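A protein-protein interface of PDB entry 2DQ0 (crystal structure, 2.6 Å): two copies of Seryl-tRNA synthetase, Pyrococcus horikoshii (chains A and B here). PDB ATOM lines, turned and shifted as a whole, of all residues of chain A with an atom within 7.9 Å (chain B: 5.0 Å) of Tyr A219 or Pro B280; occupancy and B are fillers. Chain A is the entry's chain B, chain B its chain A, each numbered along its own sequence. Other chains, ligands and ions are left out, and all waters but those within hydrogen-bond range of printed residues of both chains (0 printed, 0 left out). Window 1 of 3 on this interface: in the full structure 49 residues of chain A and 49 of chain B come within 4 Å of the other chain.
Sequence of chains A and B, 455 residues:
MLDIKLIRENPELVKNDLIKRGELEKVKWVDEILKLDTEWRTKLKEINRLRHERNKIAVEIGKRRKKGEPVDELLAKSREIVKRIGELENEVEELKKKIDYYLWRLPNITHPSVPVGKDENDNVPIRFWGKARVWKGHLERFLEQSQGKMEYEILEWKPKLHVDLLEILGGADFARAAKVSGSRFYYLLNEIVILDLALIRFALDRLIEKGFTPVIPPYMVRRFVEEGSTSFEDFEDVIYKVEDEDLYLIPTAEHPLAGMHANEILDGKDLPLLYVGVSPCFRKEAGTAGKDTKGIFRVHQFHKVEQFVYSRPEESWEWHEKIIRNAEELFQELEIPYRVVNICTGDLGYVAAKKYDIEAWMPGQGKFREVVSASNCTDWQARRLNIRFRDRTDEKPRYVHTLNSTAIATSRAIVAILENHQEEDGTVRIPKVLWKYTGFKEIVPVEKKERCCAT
Of the printed residues of chain B, Pro A218 touches Gln B301. Tyr A219 touches just these residues of chain B: Pro B280 (3.8 Å), Phe B282 (3.9 Å), Gln B301 (2.6 Å) and His B303 (2.6 Å). Leu A247 touches none of the printed residues of chain B. Pro A256 touches none of the printed residues of chain B. Of the printed residues of chain B, His A303 touches Tyr B219 (2.5 Å). Of chain A, only Tyr A219 comes within 4 Å of Pro B280. Of the printed residues of chain A, Phe B282 touches Tyr A219. Of the printed residues of chain A, Gln B301 touches Pro A217, Pro A218 and Tyr A219. Printed residues of chain A within 4 Å of His B303: Tyr A219 (2.6 Å). The nearest printed residue of chain B that does not touch Tyr A219 is Phe B302 (6.2 Å). The nearest printed residue of chain B that does not touch Pro A280 is Pro B280 (4.3 Å).
Pro A218 touches Gln B301 (C to OE1, 3.5 Å). CB of Pro B280 touches CE1 of Tyr A219, 3.8 Å away. Tyr A219 touches Phe B282 (CD1 to CE2, 3.9 Å). Tyr B219 touches Pro A280.
Tyr A219 touches Pro B280, and with the chains exchanged Pro A280 touches Tyr B219. Tyr A219 touches Phe B282, but with the chains exchanged Phe A282 does not touch Tyr B219 (4.03 Å). Tyr A219 touches Gln B301, and with the chains exchanged Gln A301 touches Tyr B219. Tyr A219 touches His B303, and with the chains exchanged His A303 touches Tyr B219.
Of the 24 printed residues of chain A, 6 touch a printed residue of chain B. Hydrophobic or aromatic side chains of chain A that line the printed part of chain B: Tyr A219, Pro A280 and His A303. Hydrophobic or aromatic side chains of chain B that line the printed part of chain A: Tyr B219, Pro B280, Phe B282 and His B303. Along chain B the printed residues that touch a printed residue of chain A span positions 219 to 303. Among the printed residues, no Asp or Glu carboxylate lies within 4 Å of a Lys or Arg side-chain nitrogen of the other chain.
The backbone NH of Ile A250 is in hydrogen-bond range of the backbone carbonyl oxygen of Tyr A219, at 2.8 Å. The backbone carbonyl oxygen (O) of Tyr B219 sits at hydrogen-bond distance from the backbone NH (N) of Ile B250 (2.9 Å). The backbone carbonyl oxygen (O) of Ile B250 sits at hydrogen-bond distance from the backbone NH (N) of Phe B282 (3.0 Å).
NE2 of His B303 lies within hydrogen-bond range of OH of Tyr A219 (2.6 Å). The side-chain amide nitrogen of Gln B301 is in hydrogen-bond range of the backbone carbonyl oxygen of Pro A217, at 3.0 Å. OE1 of Gln B301 lies within hydrogen-bond range of N of Tyr A219. The backbone NH (N) of Tyr B219 lies within hydrogen-bond range of the side-chain amide oxygen (OE1) of Gln A301, 2.5 Å away. A ring nitrogen (NE2) of His A303 sits at hydrogen-bond distance from the side-chain hydroxyl of Tyr B219 (2.5 Å).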
ATOM      1  N   VAL A 215     -13.940  12.281  26.488  1.00  0.00           N
ATOM      2  CA  VAL A 215     -13.242  13.067  25.485  1.00  0.00           C
ATOM      3  C   VAL A 215     -14.032  13.341  24.211  1.00  0.00           C
ATOM      4  O   VAL A 215     -14.832  12.516  23.773  1.00  0.00           O
ATOM      5  CB  VAL A 215     -11.854  12.397  25.135  1.00  0.00           C
ATOM      6  CG1 VAL A 215     -11.886  10.963  25.498  1.00  0.00           C
ATOM      7  CG2 VAL A 215     -11.497  12.563  23.650  1.00  0.00           C
ATOM      8  N   ILE A 216     -13.828  14.539  23.665  1.00  0.00           N
ATOM      9  CA  ILE A 216     -14.433  14.951  22.401  1.00  0.00           C
ATOM     10  C   ILE A 216     -13.190  15.139  21.542  1.00  0.00           C
ATOM     11  O   ILE A 216     -12.427  16.079  21.736  1.00  0.00           O
ATOM     12  CB  ILE A 216     -15.195  16.296  22.501  1.00  0.00           C
ATOM     13  CG1 ILE A 216     -16.517  16.095  23.240  1.00  0.00           C
ATOM     14  CG2 ILE A 216     -15.471  16.838  21.099  1.00  0.00           C
ATOM     15  CD1 ILE A 216     -17.267  17.409  23.534  1.00  0.00           C
ATOM     16  N   PRO A 217     -12.971  14.242  20.585  1.00  0.00           N
ATOM     17  CA  PRO A 217     -11.818  14.267  19.684  1.00  0.00           C
ATOM     18  C   PRO A 217     -11.989  15.087  18.434  1.00  0.00           C
ATOM     19  O   PRO A 217     -13.024  15.721  18.201  1.00  0.00           O
ATOM     20  CB  PRO A 217     -11.687  12.815  19.299  1.00  0.00           C
ATOM     21  CG  PRO A 217     -13.145  12.488  19.038  1.00  0.00           C
ATOM     22  CD  PRO A 217     -13.831  13.083  20.272  1.00  0.00           C
ATOM     23  N   PRO A 218     -10.935  15.114  17.621  1.00  0.00           N
ATOM     24  CA  PRO A 218     -11.050  15.861  16.371  1.00  0.00           C
ATOM     25  C   PRO A 218     -11.911  14.928  15.518  1.00  0.00           C
ATOM     26  O   PRO A 218     -11.795  13.695  15.647  1.00  0.00           O
ATOM     27  CB  PRO A 218      -9.612  15.924  15.883  1.00  0.00           C
ATOM     28  CG  PRO A 218      -8.862  16.046  17.178  1.00  0.00           C
ATOM     29  CD  PRO A 218      -9.518  14.966  18.008  1.00  0.00           C
ATOM     30  N   TYR A 219     -12.775  15.495  14.676  1.00  0.00           N
ATOM     31  CA  TYR A 219     -13.628  14.681  13.837  1.00  0.00           C
ATOM     32  C   TYR A 219     -12.983  14.424  12.485  1.00  0.00           C
ATOM     33  O   TYR A 219     -13.490  13.621  11.691  1.00  0.00           O
ATOM     34  CB  TYR A 219     -14.981  15.352  13.654  1.00  0.00           C
ATOM     35  CG  TYR A 219     -15.689  15.646  14.951  1.00  0.00           C
ATOM     36  CD1 TYR A 219     -16.764  16.544  14.994  1.00  0.00           C
ATOM     37  CD2 TYR A 219     -15.314  15.014  16.137  1.00  0.00           C
ATOM     38  CE1 TYR A 219     -17.443  16.794  16.166  1.00  0.00           C
ATOM     39  CE2 TYR A 219     -15.990  15.268  17.320  1.00  0.00           C
ATOM     40  CZ  TYR A 219     -17.055  16.155  17.324  1.00  0.00           C
ATOM     41  OH  TYR A 219     -17.731  16.398  18.488  1.00  0.00           O
ATOM     42  N   MET A 220     -11.876  15.124  12.227  1.00  0.00           N
ATOM     43  CA  MET A 220     -11.079  14.979  10.985  1.00  0.00           C
ATOM     44  C   MET A 220      -9.644  14.666  11.398  1.00  0.00           C
ATOM     45  O   MET A 220      -9.072  15.348  12.254  1.00  0.00           O
ATOM     46  CB  MET A 220     -11.071  16.274  10.151  1.00  0.00           C
ATOM     47  CG  MET A 220     -12.381  16.619   9.445  1.00  0.00           C
ATOM     48  SD  MET A 220     -12.437  18.356   8.946  1.00  0.00           S
ATOM     49  CE  MET A 220     -12.110  18.256   7.264  1.00  0.00           C
ATOM     50  N   VAL A 221      -9.055  13.638  10.809  1.00  0.00           N
ATOM     51  CA  VAL A 221      -7.673  13.287  11.161  1.00  0.00           C
ATOM     52  C   VAL A 221      -6.784  13.112   9.931  1.00  0.00           C
ATOM     53  O   VAL A 221      -7.281  12.951   8.816  1.00  0.00           O
ATOM     54  CB  VAL A 221      -7.607  11.966  11.930  1.00  0.00           C
ATOM     55  CG1 VAL A 221      -8.273  12.106  13.272  1.00  0.00           C
ATOM     56  CG2 VAL A 221      -8.268  10.878  11.099  1.00  0.00           C
ATOM     57  N   GLU A 226      -5.598   7.157  10.373  1.00  0.00           N
ATOM     58  CA  GLU A 226      -6.514   6.184   9.804  1.00  0.00           C
ATOM     59  C   GLU A 226      -5.773   4.894   9.443  1.00  0.00           C
ATOM     60  O   GLU A 226      -6.253   3.799   9.756  1.00  0.00           O
ATOM     61  CB  GLU A 226      -7.226   6.759   8.580  1.00  0.00           C
ATOM     62  CG  GLU A 226      -8.246   7.828   8.963  1.00  0.00           C
ATOM     63  CD  GLU A 226      -9.185   7.313  10.028  1.00  0.00           C
ATOM     64  OE1 GLU A 226      -9.975   6.381   9.742  1.00  0.00           O
ATOM     65  OE2 GLU A 226      -9.117   7.825  11.156  1.00  0.00           O
ATOM     66  N   TYR A 240     -14.339   8.926   4.297  1.00  0.00           N
ATOM     67  CA  TYR A 240     -14.427  10.100   3.420  1.00  0.00           C
ATOM     68  C   TYR A 240     -13.161  10.936   3.560  1.00  0.00           C
ATOM     69  O   TYR A 240     -12.730  11.227   4.682  1.00  0.00           O
ATOM     70  CB  TYR A 240     -15.604  11.005   3.818  1.00  0.00           C
ATOM     71  CG  TYR A 240     -16.982  10.470   3.521  1.00  0.00           C
ATOM     72  CD1 TYR A 240     -17.547  10.575   2.237  1.00  0.00           C
ATOM     73  CD2 TYR A 240     -17.745   9.886   4.533  1.00  0.00           C
ATOM     74  CE1 TYR A 240     -18.838  10.112   1.981  1.00  0.00           C
ATOM     75  CE2 TYR A 240     -19.029   9.421   4.288  1.00  0.00           C
ATOM     76  CZ  TYR A 240     -19.571   9.531   3.015  1.00  0.00           C
ATOM     77  OH  TYR A 240     -20.818   9.014   2.795  1.00  0.00           O
ATOM     78  N   LEU A 247      -6.668  15.353   5.582  1.00  0.00           N
ATOM     79  CA  LEU A 247      -7.700  15.241   6.593  1.00  0.00           C
ATOM     80  C   LEU A 247      -8.724  14.196   6.124  1.00  0.00           C
ATOM     81  O   LEU A 247      -9.028  14.099   4.938  1.00  0.00           O
ATOM     82  CB  LEU A 247      -8.393  16.584   6.825  1.00  0.00           C
ATOM     83  CG  LEU A 247      -7.581  17.700   7.477  1.00  0.00           C
ATOM     84  CD1 LEU A 247      -8.416  18.942   7.465  1.00  0.00           C
ATOM     85  CD2 LEU A 247      -7.178  17.318   8.902  1.00  0.00           C
ATOM     86  N   TYR A 248      -9.221  13.400   7.067  1.00  0.00           N
ATOM     87  CA  TYR A 248     -10.213  12.369   6.800  1.00  0.00           C
ATOM     88  C   TYR A 248     -11.277  12.428   7.881  1.00  0.00           C
ATOM     89  O   TYR A 248     -10.976  12.657   9.048  1.00  0.00           O
ATOM     90  CB  TYR A 248      -9.572  10.984   6.802  1.00  0.00           C
ATOM     91  CG  TYR A 248      -8.517  10.845   5.767  1.00  0.00           C
ATOM     92  CD1 TYR A 248      -7.292  11.512   5.915  1.00  0.00           C
ATOM     93  CD2 TYR A 248      -8.752  10.113   4.591  1.00  0.00           C
ATOM     94  CE1 TYR A 248      -6.322  11.473   4.931  1.00  0.00           C
ATOM     95  CE2 TYR A 248      -7.777  10.055   3.579  1.00  0.00           C
ATOM     96  CZ  TYR A 248      -6.564  10.745   3.763  1.00  0.00           C
ATOM     97  OH  TYR A 248      -5.596  10.738   2.798  1.00  0.00           O
ATOM     98  N   LEU A 249     -12.523  12.240   7.470  1.00  0.00           N
ATOM     99  CA  LEU A 249     -13.658  12.267   8.378  1.00  0.00           C
ATOM    100  C   LEU A 249     -13.633  10.996   9.187  1.00  0.00           C
ATOM    101  O   LEU A 249     -13.512   9.899   8.632  1.00  0.00           O
ATOM    102  CB  LEU A 249     -14.948  12.403   7.572  1.00  0.00           C
ATOM    103  CG  LEU A 249     -15.151  13.844   7.072  1.00  0.00           C
ATOM    104  CD1 LEU A 249     -16.348  13.960   6.157  1.00  0.00           C
ATOM    105  CD2 LEU A 249     -15.377  14.723   8.280  1.00  0.00           C
ATOM    106  N   ILE A 250     -13.733  11.119  10.505  1.00  0.00           N
ATOM    107  CA  ILE A 250     -13.642   9.901  11.305  1.00  0.00           C
ATOM    108  C   ILE A 250     -14.898   9.041  11.271  1.00  0.00           C
ATOM    109  O   ILE A 250     -16.015   9.544  11.336  1.00  0.00           O
ATOM    110  CB  ILE A 250     -13.253  10.202  12.768  1.00  0.00           C
ATOM    111  CG1 ILE A 250     -14.419  10.876  13.498  1.00  0.00           C
ATOM    112  CG2 ILE A 250     -11.982  11.061  12.784  1.00  0.00           C
ATOM    113  CD1 ILE A 250     -14.228  10.923  14.951  1.00  0.00           C
ATOM    114  N   PRO A 251     -14.721   7.721  11.144  1.00  0.00           N
ATOM    115  CA  PRO A 251     -15.840   6.776  11.099  1.00  0.00           C
ATOM    116  C   PRO A 251     -16.247   6.310  12.497  1.00  0.00           C
ATOM    117  O   PRO A 251     -17.238   5.629  12.656  1.00  0.00           O
ATOM    118  CB  PRO A 251     -15.281   5.635  10.257  1.00  0.00           C
ATOM    119  CG  PRO A 251     -13.838   5.587  10.711  1.00  0.00           C
ATOM    120  CD  PRO A 251     -13.444   7.053  10.817  1.00  0.00           C
ATOM    121  N   THR A 252     -15.464   6.696  13.497  1.00  0.00           N
ATOM    122  CA  THR A 252     -15.698   6.310  14.882  1.00  0.00           C
ATOM    123  C   THR A 252     -14.649   6.993  15.755  1.00  0.00           C
ATOM    124  O   THR A 252     -13.515   7.168  15.302  1.00  0.00           O
ATOM    125  CB  THR A 252     -15.549   4.764  15.072  1.00  0.00           C
ATOM    126  OG1 THR A 252     -15.308   4.468  16.453  1.00  0.00           O
ATOM    127  CG2 THR A 252     -14.384   4.209  14.245  1.00  0.00           C
ATOM    128  N   ALA A 253     -15.018   7.370  16.987  1.00  0.00           N
ATOM    129  CA  ALA A 253     -14.069   7.997  17.916  1.00  0.00           C
ATOM    130  C   ALA A 253     -12.864   7.089  18.203  1.00  0.00           C
ATOM    131  O   ALA A 253     -11.833   7.548  18.671  1.00  0.00           O
ATOM    132  CB  ALA A 253     -14.747   8.366  19.214  1.00  0.00           C
ATOM    133  N   PRO A 256      -9.398   8.587  16.296  1.00  0.00           N
ATOM    134  CA  PRO A 256      -8.604   9.647  16.927  1.00  0.00           C
ATOM    135  C   PRO A 256      -8.140   9.233  18.321  1.00  0.00           C
ATOM    136  O   PRO A 256      -7.083   9.668  18.795  1.00  0.00           O
ATOM    137  CB  PRO A 256      -9.561  10.846  16.947  1.00  0.00           C
ATOM    138  CG  PRO A 256     -10.925  10.220  16.858  1.00  0.00           C
ATOM    139  CD  PRO A 256     -10.727   9.089  15.906  1.00  0.00           C
ATOM    140  N   VAL A 278     -16.923  10.769  22.571  1.00  0.00           N
ATOM    141  CA  VAL A 278     -18.231  11.051  21.971  1.00  0.00           C
ATOM    142  C   VAL A 278     -17.917  11.709  20.648  1.00  0.00           C
ATOM    143  O   VAL A 278     -16.973  12.496  20.562  1.00  0.00           O
ATOM    144  CB  VAL A 278     -19.061  12.138  22.679  1.00  0.00           C
ATOM    145  CG1 VAL A 278     -20.506  11.937  22.331  1.00  0.00           C
ATOM    146  CG2 VAL A 278     -18.820  12.173  24.136  1.00  0.00           C
ATOM    147  N   SER A 279     -18.708  11.430  19.623  1.00  0.00           N
ATOM    148  CA  SER A 279     -18.468  12.102  18.354  1.00  0.00           C
ATOM    149  C   SER A 279     -19.401  11.660  17.250  1.00  0.00           C
ATOM    150  O   SER A 279     -20.036  10.595  17.315  1.00  0.00           O
ATOM    151  CB  SER A 279     -17.027  11.874  17.856  1.00  0.00           C
ATOM    152  OG  SER A 279     -16.904  10.636  17.145  1.00  0.00           O
ATOM    153  N   PRO A 280     -19.550  12.514  16.243  1.00  0.00           N
ATOM    154  CA  PRO A 280     -20.409  12.089  15.147  1.00  0.00           C
ATOM    155  C   PRO A 280     -19.452  11.144  14.413  1.00  0.00           C
ATOM    156  O   PRO A 280     -18.233  11.207  14.632  1.00  0.00           O
ATOM    157  CB  PRO A 280     -20.663  13.382  14.364  1.00  0.00           C
ATOM    158  CG  PRO A 280     -19.437  14.213  14.681  1.00  0.00           C
ATOM    159  CD  PRO A 280     -19.211  13.940  16.143  1.00  0.00           C
ATOM    160  N   CYS A 281     -20.018  10.280  13.576  1.00  0.00           N
ATOM    161  CA  CYS A 281     -19.287   9.290  12.786  1.00  0.00           C
ATOM    162  C   CYS A 281     -19.729   9.322  11.334  1.00  0.00           C
ATOM    163  O   CYS A 281     -20.918   9.380  11.043  1.00  0.00           O
ATOM    164  CB  CYS A 281     -19.552   7.892  13.320  1.00  0.00           C
ATOM    165  SG  CYS A 281     -18.948   7.591  14.951  1.00  0.00           S
ATOM    166  N   PHE A 282     -18.766   9.230  10.435  1.00  0.00           N
ATOM    167  CA  PHE A 282     -19.038   9.255   9.019  1.00  0.00           C
ATOM    168  C   PHE A 282     -18.555   8.023   8.257  1.00  0.00           C
ATOM    169  O   PHE A 282     -17.393   7.670   8.327  1.00  0.00           O
ATOM    170  CB  PHE A 282     -18.407  10.501   8.433  1.00  0.00           C
ATOM    171  CG  PHE A 282     -18.714  11.747   9.207  1.00  0.00           C
ATOM    172  CD1 PHE A 282     -17.893  12.147  10.264  1.00  0.00           C
ATOM    173  CD2 PHE A 282     -19.821  12.526   8.879  1.00  0.00           C
ATOM    174  CE1 PHE A 282     -18.173  13.295  10.970  1.00  0.00           C
ATOM    175  CE2 PHE A 282     -20.111  13.681   9.587  1.00  0.00           C
ATOM    176  CZ  PHE A 282     -19.290  14.072  10.633  1.00  0.00           C
ATOM    177  N   GLN A 301     -24.120   9.101   8.515  1.00  0.00           N
ATOM    178  CA  GLN A 301     -23.830   9.941   9.660  1.00  0.00           C
ATOM    179  C   GLN A 301     -24.560   9.514  10.937  1.00  0.00           C
ATOM    180  O   GLN A 301     -25.784   9.413  10.966  1.00  0.00           O
ATOM    181  CB  GLN A 301     -24.175  11.406   9.264  1.00  0.00           C
ATOM    182  CG  GLN A 301     -24.520  12.375  10.385  1.00  0.00           C
ATOM    183  CD  GLN A 301     -25.050  13.729   9.896  1.00  0.00           C
ATOM    184  OE1 GLN A 301     -24.701  14.195   8.821  1.00  0.00           O
ATOM    185  NE2 GLN A 301     -25.883  14.370  10.708  1.00  0.00           N
ATOM    186  N   HIS A 303     -24.176   9.259  15.615  1.00  0.00           N
ATOM    187  CA  HIS A 303     -23.507   9.609  16.840  1.00  0.00           C
ATOM    188  C   HIS A 303     -23.173   8.342  17.613  1.00  0.00           C
ATOM    189  O   HIS A 303     -23.969   7.419  17.665  1.00  0.00           O
ATOM    190  CB  HIS A 303     -24.422  10.510  17.673  1.00  0.00           C
ATOM    191  CG  HIS A 303     -24.743  11.817  17.020  1.00  0.00           C
ATOM    192  ND1 HIS A 303     -25.768  12.633  17.452  1.00  0.00           N
ATOM    193  CD2 HIS A 303     -24.142  12.480  16.005  1.00  0.00           C
ATOM    194  CE1 HIS A 303     -25.785  13.741  16.733  1.00  0.00           C
ATOM    195  NE2 HIS A 303     -24.808  13.675  15.847  1.00  0.00           N
ATOM    196  N   TYR B 219     -24.891  16.624   8.203  1.00  0.00           N
ATOM    197  CA  TYR B 219     -23.704  17.425   8.490  1.00  0.00           C
ATOM    198  C   TYR B 219     -22.926  17.667   7.200  1.00  0.00           C
ATOM    199  O   TYR B 219     -21.984  18.463   7.164  1.00  0.00           O
ATOM    200  CB  TYR B 219     -22.826  16.689   9.507  1.00  0.00           C
ATOM    201  CG  TYR B 219     -23.491  16.463  10.857  1.00  0.00           C
ATOM    202  CD1 TYR B 219     -23.051  15.440  11.705  1.00  0.00           C
ATOM    203  CD2 TYR B 219     -24.543  17.276  11.291  1.00  0.00           C
ATOM    204  CE1 TYR B 219     -23.645  15.225  12.955  1.00  0.00           C
ATOM    205  CE2 TYR B 219     -25.145  17.077  12.546  1.00  0.00           C
ATOM    206  CZ  TYR B 219     -24.685  16.045  13.362  1.00  0.00           C
ATOM    207  OH  TYR B 219     -25.269  15.812  14.574  1.00  0.00           O
ATOM    208  N   ILE B 250     -20.897  21.105   6.576  1.00  0.00           N
ATOM    209  CA  ILE B 250     -21.584  22.336   6.904  1.00  0.00           C
ATOM    210  C   ILE B 250     -20.798  23.183   7.887  1.00  0.00           C
ATOM    211  O   ILE B 250     -20.148  22.663   8.787  1.00  0.00           O
ATOM    212  CB  ILE B 250     -22.990  22.049   7.478  1.00  0.00           C
ATOM    213  CG1 ILE B 250     -22.885  21.236   8.761  1.00  0.00           C
ATOM    214  CG2 ILE B 250     -23.818  21.243   6.474  1.00  0.00           C
ATOM    215  CD1 ILE B 250     -24.204  21.104   9.460  1.00  0.00           C
ATOM    216  N   VAL B 278     -28.986  21.593  16.078  1.00  0.00           N
ATOM    217  CA  VAL B 278     -27.755  21.311  16.821  1.00  0.00           C
ATOM    218  C   VAL B 278     -26.906  20.611  15.789  1.00  0.00           C
ATOM    219  O   VAL B 278     -27.417  19.804  15.013  1.00  0.00           O
ATOM    220  CB  VAL B 278     -27.898  20.251  17.946  1.00  0.00           C
ATOM    221  CG1 VAL B 278     -26.796  20.446  18.975  1.00  0.00           C
ATOM    222  CG2 VAL B 278     -29.247  20.293  18.548  1.00  0.00           C
ATOM    223  N   SER B 279     -25.614  20.897  15.778  1.00  0.00           N
ATOM    224  CA  SER B 279     -24.746  20.225  14.836  1.00  0.00           C
ATOM    225  C   SER B 279     -23.314  20.639  15.004  1.00  0.00           C
ATOM    226  O   SER B 279     -23.031  21.710  15.525  1.00  0.00           O
ATOM    227  CB  SER B 279     -25.148  20.544  13.394  1.00  0.00           C
ATOM    228  OG  SER B 279     -24.447  21.681  12.914  1.00  0.00           O
ATOM    229  N   PRO B 280     -22.385  19.762  14.615  1.00  0.00           N
ATOM    230  CA  PRO B 280     -21.007  20.209  14.753  1.00  0.00           C
ATOM    231  C   PRO B 280     -20.866  21.165  13.557  1.00  0.00           C
ATOM    232  O   PRO B 280     -21.727  21.186  12.674  1.00  0.00           O
ATOM    233  CB  PRO B 280     -20.194  18.909  14.616  1.00  0.00           C
ATOM    234  CG  PRO B 280     -21.076  18.030  13.780  1.00  0.00           C
ATOM    235  CD  PRO B 280     -22.457  18.320  14.320  1.00  0.00           C
ATOM    236  N   CYS B 281     -19.818  21.979  13.548  1.00  0.00           N
ATOM    237  CA  CYS B 281     -19.586  22.928  12.462  1.00  0.00           C
ATOM    238  C   CYS B 281     -18.147  22.843  12.029  1.00  0.00           C
ATOM    239  O   CYS B 281     -17.248  22.760  12.871  1.00  0.00           O
ATOM    240  CB  CYS B 281     -19.881  24.358  12.920  1.00  0.00           C
ATOM    241  SG  CYS B 281     -21.566  24.631  13.500  1.00  0.00           S
ATOM    242  N   PHE B 282     -17.919  22.893  10.720  1.00  0.00           N
ATOM    243  CA  PHE B 282     -16.568  22.801  10.190  1.00  0.00           C
ATOM    244  C   PHE B 282     -16.240  23.986   9.322  1.00  0.00           C
ATOM    245  O   PHE B 282     -16.987  24.311   8.401  1.00  0.00           O
ATOM    246  CB  PHE B 282     -16.403  21.510   9.381  1.00  0.00           C
ATOM    247  CG  PHE B 282     -16.912  20.297  10.079  1.00  0.00           C
ATOM    248  CD1 PHE B 282     -18.266  19.955  10.006  1.00  0.00           C
ATOM    249  CD2 PHE B 282     -16.062  19.510  10.848  1.00  0.00           C
ATOM    250  CE1 PHE B 282     -18.763  18.850  10.690  1.00  0.00           C
ATOM    251  CE2 PHE B 282     -16.549  18.389  11.544  1.00  0.00           C
ATOM    252  CZ  PHE B 282     -17.902  18.061  11.465  1.00  0.00           C
ATOM    253  N   GLN B 301     -13.370  22.933  14.122  1.00  0.00           N
ATOM    254  CA  GLN B 301     -14.636  22.287  14.461  1.00  0.00           C
ATOM    255  C   GLN B 301     -15.148  22.749  15.814  1.00  0.00           C
ATOM    256  O   GLN B 301     -14.379  22.911  16.766  1.00  0.00           O
ATOM    257  CB  GLN B 301     -14.522  20.743  14.457  1.00  0.00           C
ATOM    258  CG  GLN B 301     -13.962  20.150  15.712  1.00  0.00           C
ATOM    259  CD  GLN B 301     -13.888  18.612  15.724  1.00  0.00           C
ATOM    260  OE1 GLN B 301     -13.360  17.991  14.795  1.00  0.00           O
ATOM    261  NE2 GLN B 301     -14.376  18.004  16.811  1.00  0.00           N
ATOM    262  N   PHE B 302     -16.453  22.983  15.867  1.00  0.00           N
ATOM    263  CA  PHE B 302     -17.141  23.385  17.086  1.00  0.00           C
ATOM    264  C   PHE B 302     -18.616  23.019  17.000  1.00  0.00           C
ATOM    265  O   PHE B 302     -19.174  22.787  15.908  1.00  0.00           O
ATOM    266  CB  PHE B 302     -17.016  24.884  17.354  1.00  0.00           C
ATOM    267  CG  PHE B 302     -17.602  25.755  16.280  1.00  0.00           C
ATOM    268  CD1 PHE B 302     -16.870  26.067  15.137  1.00  0.00           C
ATOM    269  CD2 PHE B 302     -18.873  26.303  16.428  1.00  0.00           C
ATOM    270  CE1 PHE B 302     -17.396  26.918  14.163  1.00  0.00           C
ATOM    271  CE2 PHE B 302     -19.407  27.161  15.459  1.00  0.00           C
ATOM    272  CZ  PHE B 302     -18.668  27.468  14.327  1.00  0.00           C
ATOM    273  N   HIS B 303     -19.242  22.970  18.163  1.00  0.00           N
ATOM    274  CA  HIS B 303     -20.650  22.634  18.269  1.00  0.00           C
ATOM    275  C   HIS B 303     -21.475  23.908  18.399  1.00  0.00           C
ATOM    276  O   HIS B 303     -21.063  24.854  19.082  1.00  0.00           O
ATOM    277  CB  HIS B 303     -20.845  21.741  19.482  1.00  0.00           C
ATOM    278  CG  HIS B 303     -20.176  20.415  19.351  1.00  0.00           C
ATOM    279  ND1 HIS B 303     -19.810  19.654  20.440  1.00  0.00           N
ATOM    280  CD2 HIS B 303     -19.841  19.692  18.253  1.00  0.00           C
ATOM    281  CE1 HIS B 303     -19.277  18.519  20.018  1.00  0.00           C
ATOM    282  NE2 HIS B 303     -19.284  18.516  18.696  1.00  0.00           N
